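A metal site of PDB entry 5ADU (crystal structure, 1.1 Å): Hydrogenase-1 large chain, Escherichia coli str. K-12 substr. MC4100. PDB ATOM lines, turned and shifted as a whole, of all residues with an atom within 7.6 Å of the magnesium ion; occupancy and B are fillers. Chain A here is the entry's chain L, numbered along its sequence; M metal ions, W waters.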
ATOM      1  N   PHE A  53     -18.078  13.706  -2.421  1.00  0.00           N
ATOM      2  CA  PHE A  53     -17.585  14.570  -3.500  1.00  0.00           C
ATOM      3  C   PHE A  53     -17.150  13.663  -4.651  1.00  0.00           C
ATOM      4  O   PHE A  53     -16.536  12.617  -4.428  1.00  0.00           O
ATOM      5  CB  PHE A  53     -16.386  15.431  -3.022  1.00  0.00           C
ATOM      6  CG  PHE A  53     -15.734  16.267  -4.127  1.00  0.00           C
ATOM      7  CD1 PHE A  53     -16.358  17.443  -4.608  1.00  0.00           C
ATOM      8  CD2 PHE A  53     -14.532  15.880  -4.702  1.00  0.00           C
ATOM      9  CE1 PHE A  53     -15.755  18.213  -5.605  1.00  0.00           C
ATOM     10  CE2 PHE A  53     -13.931  16.659  -5.705  1.00  0.00           C
ATOM     11  CZ  PHE A  53     -14.540  17.829  -6.141  1.00  0.00           C
ATOM     12  N   GLU A  57     -16.851  19.278 -12.005  1.00  0.00           N
ATOM     13  CA  GLU A  57     -16.269  20.506 -12.573  1.00  0.00           C
ATOM     14  C   GLU A  57     -14.850  20.288 -13.139  1.00  0.00           C
ATOM     15  O   GLU A  57     -14.416  20.968 -14.088  1.00  0.00           O
ATOM     16  CB  GLU A  57     -16.269  21.645 -11.545  1.00  0.00           C
ATOM     17  CG  GLU A  57     -17.674  22.066 -11.101  1.00  0.00           C
ATOM     18  CD  GLU A  57     -17.773  22.713  -9.750  1.00  0.00           C
ATOM     19  OE1 GLU A  57     -16.927  22.351  -8.861  1.00  0.00           O
ATOM     20  OE2 GLU A  57     -18.751  23.508  -9.505  1.00  0.00           O
ATOM     21  N   GLU A 347     -18.703  32.290  -4.014  1.00  0.00           N
ATOM     22  CA  GLU A 347     -18.556  31.104  -3.135  1.00  0.00           C
ATOM     23  C   GLU A 347     -17.293  31.211  -2.278  1.00  0.00           C
ATOM     24  O   GLU A 347     -16.195  31.520  -2.792  1.00  0.00           O
ATOM     25  CB  GLU A 347     -18.552  29.807  -3.971  1.00  0.00           C
ATOM     26  CG  GLU A 347     -19.853  29.483  -4.680  1.00  0.00           C
ATOM     27  CD  GLU A 347     -19.786  28.174  -5.438  1.00  0.00           C
ATOM     28  OE1 GLU A 347     -19.020  28.123  -6.450  1.00  0.00           O
ATOM     29  OE2 GLU A 347     -20.517  27.219  -5.015  1.00  0.00           O
ATOM     30  N   TYR A 354     -11.541  22.613   0.463  1.00  0.00           N
ATOM     31  CA  TYR A 354     -11.028  23.118  -0.816  1.00  0.00           C
ATOM     32  C   TYR A 354      -9.901  24.128  -0.562  1.00  0.00           C
ATOM     33  O   TYR A 354      -9.851  24.754   0.496  1.00  0.00           O
ATOM     34  CB  TYR A 354     -12.127  23.809  -1.655  1.00  0.00           C
ATOM     35  CG  TYR A 354     -13.290  22.901  -2.025  1.00  0.00           C
ATOM     36  CD1 TYR A 354     -13.199  22.015  -3.094  1.00  0.00           C
ATOM     37  CD2 TYR A 354     -14.435  22.870  -1.278  1.00  0.00           C
ATOM     38  CE1 TYR A 354     -14.229  21.111  -3.384  1.00  0.00           C
ATOM     39  CE2 TYR A 354     -15.480  22.010  -1.528  1.00  0.00           C
ATOM     40  CZ  TYR A 354     -15.368  21.108  -2.613  1.00  0.00           C
ATOM     41  OH  TYR A 354     -16.409  20.216  -2.917  1.00  0.00           O
ATOM     42  N   PRO A 365     -18.467  32.501  -9.920  1.00  0.00           N
ATOM     43  CA  PRO A 365     -18.155  31.233 -10.635  1.00  0.00           C
ATOM     44  C   PRO A 365     -17.289  31.327 -11.880  1.00  0.00           C
ATOM     45  O   PRO A 365     -16.561  30.378 -12.199  1.00  0.00           O
ATOM     46  CB  PRO A 365     -19.560  30.626 -10.906  1.00  0.00           C
ATOM     47  CG  PRO A 365     -20.390  31.179  -9.776  1.00  0.00           C
ATOM     48  CD  PRO A 365     -19.919  32.598  -9.651  1.00  0.00           C
ATOM     49  N   ILE A 369     -12.721  27.992  -8.499  1.00  0.00           N
ATOM     50  CA  ILE A 369     -11.594  27.029  -8.340  1.00  0.00           C
ATOM     51  C   ILE A 369     -12.153  25.813  -7.599  1.00  0.00           C
ATOM     52  O   ILE A 369     -12.778  25.995  -6.533  1.00  0.00           O
ATOM     53  CB  ILE A 369     -10.384  27.613  -7.574  1.00  0.00           C
ATOM     54  CG1 ILE A 369      -9.831  28.892  -8.244  1.00  0.00           C
ATOM     55  CG2 ILE A 369      -9.260  26.583  -7.449  1.00  0.00           C
ATOM     56  CD1 ILE A 369      -8.775  29.625  -7.409  1.00  0.00           C
ATOM     57  N   THR A 370     -11.910  24.618  -8.122  1.00  0.00           N
ATOM     58  CA  THR A 370     -12.292  23.374  -7.433  1.00  0.00           C
ATOM     59  C   THR A 370     -11.033  22.501  -7.270  1.00  0.00           C
ATOM     60  O   THR A 370     -10.716  21.671  -8.163  1.00  0.00           O
ATOM     61  CB  THR A 370     -13.429  22.644  -8.174  1.00  0.00           C
ATOM     62  OG1 THR A 370     -14.515  23.574  -8.324  1.00  0.00           O
ATOM     63  CG2 THR A 370     -13.906  21.407  -7.377  1.00  0.00           C
ATOM     64  N   LYS A 399     -19.317  23.887  -0.848  1.00  0.00           N
ATOM     65  CA  LYS A 399     -18.870  25.302  -0.802  1.00  0.00           C
ATOM     66  C   LYS A 399     -19.964  26.204  -0.210  1.00  0.00           C
ATOM     67  O   LYS A 399     -21.154  25.777  -0.107  1.00  0.00           O
ATOM     68  CB  LYS A 399     -18.506  25.795  -2.230  1.00  0.00           C
ATOM     69  CG  LYS A 399     -17.351  25.069  -2.947  1.00  0.00           C
ATOM     70  CD  LYS A 399     -16.997  25.750  -4.271  1.00  0.00           C
ATOM     71  CE  LYS A 399     -15.849  25.096  -5.022  1.00  0.00           C
ATOM     72  NZ  LYS A 399     -15.795  25.552  -6.442  1.00  0.00           N
ATOM     73  N   GLY A 513     -27.511  27.363 -11.320  1.00  0.00           N
ATOM     74  CA  GLY A 513     -26.732  27.991 -12.383  1.00  0.00           C
ATOM     75  C   GLY A 513     -25.510  27.148 -12.779  1.00  0.00           C
ATOM     76  O   GLY A 513     -24.861  26.502 -11.923  1.00  0.00           O
ATOM     77  N   TYR A 526     -15.843  25.046 -16.123  1.00  0.00           N
ATOM     78  CA  TYR A 526     -17.259  24.676 -15.941  1.00  0.00           C
ATOM     79  C   TYR A 526     -17.521  24.684 -14.439  1.00  0.00           C
ATOM     80  O   TYR A 526     -17.017  23.778 -13.733  1.00  0.00           O
ATOM     81  CB  TYR A 526     -17.544  23.307 -16.593  1.00  0.00           C
ATOM     82  CG  TYR A 526     -19.023  23.109 -16.962  1.00  0.00           C
ATOM     83  CD1 TYR A 526     -20.008  22.953 -16.003  1.00  0.00           C
ATOM     84  CD2 TYR A 526     -19.449  23.175 -18.311  1.00  0.00           C
ATOM     85  CE1 TYR A 526     -21.365  22.848 -16.337  1.00  0.00           C
ATOM     86  CE2 TYR A 526     -20.812  23.050 -18.657  1.00  0.00           C
ATOM     87  CZ  TYR A 526     -21.756  22.877 -17.681  1.00  0.00           C
ATOM     88  OH  TYR A 526     -23.104  22.776 -18.051  1.00  0.00           O
ATOM     89  N   GLN A 527     -18.279  25.674 -13.936  1.00  0.00           N
ATOM     90  CA  GLN A 527     -18.541  25.822 -12.517  1.00  0.00           C
ATOM     91  C   GLN A 527     -20.072  25.776 -12.282  1.00  0.00           C
ATOM     92  O   GLN A 527     -20.855  26.477 -12.956  1.00  0.00           O
ATOM     93  CB  GLN A 527     -17.919  27.110 -11.945  1.00  0.00           C
ATOM     94  CG  GLN A 527     -16.401  27.004 -11.850  1.00  0.00           C
ATOM     95  CD  GLN A 527     -15.937  26.178 -10.628  1.00  0.00           C
ATOM     96  OE1 GLN A 527     -16.548  26.201  -9.559  1.00  0.00           O
ATOM     97  NE2 GLN A 527     -14.829  25.465 -10.782  1.00  0.00           N
ATOM     98  N   CYS A 528     -20.485  24.971 -11.292  1.00  0.00           N
ATOM     99  CA  CYS A 528     -21.891  24.809 -10.938  1.00  0.00           C
ATOM    100  C   CYS A 528     -22.140  25.304  -9.512  1.00  0.00           C
ATOM    101  O   CYS A 528     -21.361  25.009  -8.585  1.00  0.00           O
ATOM    102  CB  CYS A 528     -22.346  23.314 -11.018  1.00  0.00           C
ATOM    103  SG  CYS A 528     -22.023  22.506 -12.625  1.00  0.00           S
ATOM    104  N   VAL A 529     -23.273  25.981  -9.311  1.00  0.00           N
ATOM    105  CA  VAL A 529     -23.765  26.358  -7.981  1.00  0.00           C
ATOM    106  C   VAL A 529     -25.232  25.873  -7.959  1.00  0.00           C
ATOM    107  O   VAL A 529     -26.030  26.290  -8.810  1.00  0.00           O
ATOM    108  CB  VAL A 529     -23.676  27.875  -7.670  1.00  0.00           C
ATOM    109  CG1 VAL A 529     -24.053  28.117  -6.209  1.00  0.00           C
ATOM    110  CG2 VAL A 529     -22.312  28.453  -7.981  1.00  0.00           C
ATOM    111  N   VAL A 530     -25.565  24.935  -7.043  1.00  0.00           N
ATOM    112  CA  VAL A 530     -26.789  24.134  -7.127  1.00  0.00           C
ATOM    113  C   VAL A 530     -27.686  24.468  -5.904  1.00  0.00           C
ATOM    114  O   VAL A 530     -27.169  24.943  -4.891  1.00  0.00           O
ATOM    115  CB  VAL A 530     -26.348  22.635  -7.234  1.00  0.00           C
ATOM    116  CG1 VAL A 530     -27.469  21.684  -7.491  1.00  0.00           C
ATOM    117  CG2 VAL A 530     -25.307  22.461  -8.355  1.00  0.00           C
ATOM    118  N   THR A 533     -26.492  23.322  -2.567  1.00  0.00           N
ATOM    119  CA  THR A 533     -25.256  24.054  -2.204  1.00  0.00           C
ATOM    120  C   THR A 533     -25.589  25.313  -1.335  1.00  0.00           C
ATOM    121  O   THR A 533     -24.970  25.591  -0.293  1.00  0.00           O
ATOM    122  CB  THR A 533     -24.402  24.490  -3.421  1.00  0.00           C
ATOM    123  OG1 THR A 533     -24.339  23.447  -4.428  1.00  0.00           O
ATOM    124  CG2 THR A 533     -23.008  24.924  -2.981  1.00  0.00           C
ATOM    125  N   CYS A 579     -26.291  16.633  -5.685  1.00  0.00           N
ATOM    126  CA  CYS A 579     -26.389  17.956  -6.286  1.00  0.00           C
ATOM    127  C   CYS A 579     -25.497  18.983  -5.574  1.00  0.00           C
ATOM    128  O   CYS A 579     -24.814  19.800  -6.217  1.00  0.00           O
ATOM    129  CB  CYS A 579     -27.837  18.484  -6.207  1.00  0.00           C
ATOM    130  SG  CYS A 579     -28.852  17.987  -7.622  1.00  0.00           S
ATOM    131  N   SER A 580     -25.497  18.981  -4.222  1.00  0.00           N
ATOM    132  CA  SER A 580     -24.818  20.075  -3.480  1.00  0.00           C
ATOM    133  C   SER A 580     -23.297  20.102  -3.703  1.00  0.00           C
ATOM    134  O   SER A 580     -22.693  21.188  -3.612  1.00  0.00           O
ATOM    135  CB  SER A 580     -25.104  19.954  -1.966  1.00  0.00           C
ATOM    136  OG  SER A 580     -24.401  18.911  -1.306  1.00  0.00           O
ATOM    137  N   THR A 581     -22.701  18.915  -3.898  1.00  0.00           N
ATOM    138  CA  THR A 581     -21.247  18.699  -3.948  1.00  0.00           C
ATOM    139  C   THR A 581     -20.723  18.518  -5.379  1.00  0.00           C
ATOM    140  O   THR A 581     -19.607  18.978  -5.721  1.00  0.00           O
ATOM    141  CB  THR A 581     -20.876  17.479  -3.047  1.00  0.00           C
ATOM    142  OG1 THR A 581     -21.625  16.326  -3.461  1.00  0.00           O
ATOM    143  CG2 THR A 581     -21.131  17.814  -1.550  1.00  0.00           C
ATOM    144  N   HIS A 582     -21.462  17.774  -6.227  1.00  0.00           N
ATOM    145  CA  HIS A 582     -21.105  17.532  -7.621  1.00  0.00           C
ATOM    146  C   HIS A 582     -19.609  17.161  -7.770  1.00  0.00           C
ATOM    147  O   HIS A 582     -18.949  17.692  -8.694  1.00  0.00           O
ATOM    148  CB  HIS A 582     -21.615  18.681  -8.553  1.00  0.00           C
ATOM    149  CG  HIS A 582     -21.400  20.104  -8.045  1.00  0.00           C
ATOM    150  ND1 HIS A 582     -22.278  20.703  -7.162  1.00  0.00           N
ATOM    151  CD2 HIS A 582     -20.459  21.030  -8.332  1.00  0.00           C
ATOM    152  CE1 HIS A 582     -21.846  21.946  -6.922  1.00  0.00           C
ATOM    153  NE2 HIS A 582     -20.741  22.177  -7.613  1.00  0.00           N
ATOM    154  OXT HIS A 582     -19.122  16.247  -6.992  1.00  0.00           O
HETATM  155 MG    MG M   1     -19.644  24.117  -7.630  1.00  0.00          MG
HETATM  156  O   HOH W   1     -17.999  23.254  -6.598  1.00  0.00           O
HETATM  157  O   HOH W   2     -18.579  25.910  -7.805  1.00  0.00           O
HETATM  158  O   HOH W   3     -20.477  24.670  -5.791  1.00  0.00           O
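The nearest printed residue that does not touch the magnesium ion is Glu 347 (4.2 Å).
The magnesium ion is bound by water W3 (2.1 Å), water W2 (2.1 Å), water W1 (2.1 Å), O of Cys 528 (2.2 Å), OE2 of Glu 57 (2.2 Å) and NE2 of His 582 (2.2 Å).
Water W2 lies within hydrogen-bond range of the side-chain carboxylate of Glu 347, the side-chain amide oxygen of Gln 527 and the side-chain amino group of Lys 399. Water W1 bridges the side-chain carboxylate of Glu 57 and the side-chain amino group of Lys 399.
The side-chain carboxylate (OE2) of Glu 57 lies close to the side-chain amide oxygen (OE1) of Gln 527, 3.5 Å away. OG1 of Thr 370 is in hydrogen-bond range of OE1 of Glu 57, 2.8 Å away. A ring nitrogen (ND1) of His 582 sits at hydrogen-bond distance from the backbone carbonyl oxygen (O) of Cys 579, at 2.9 Å.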
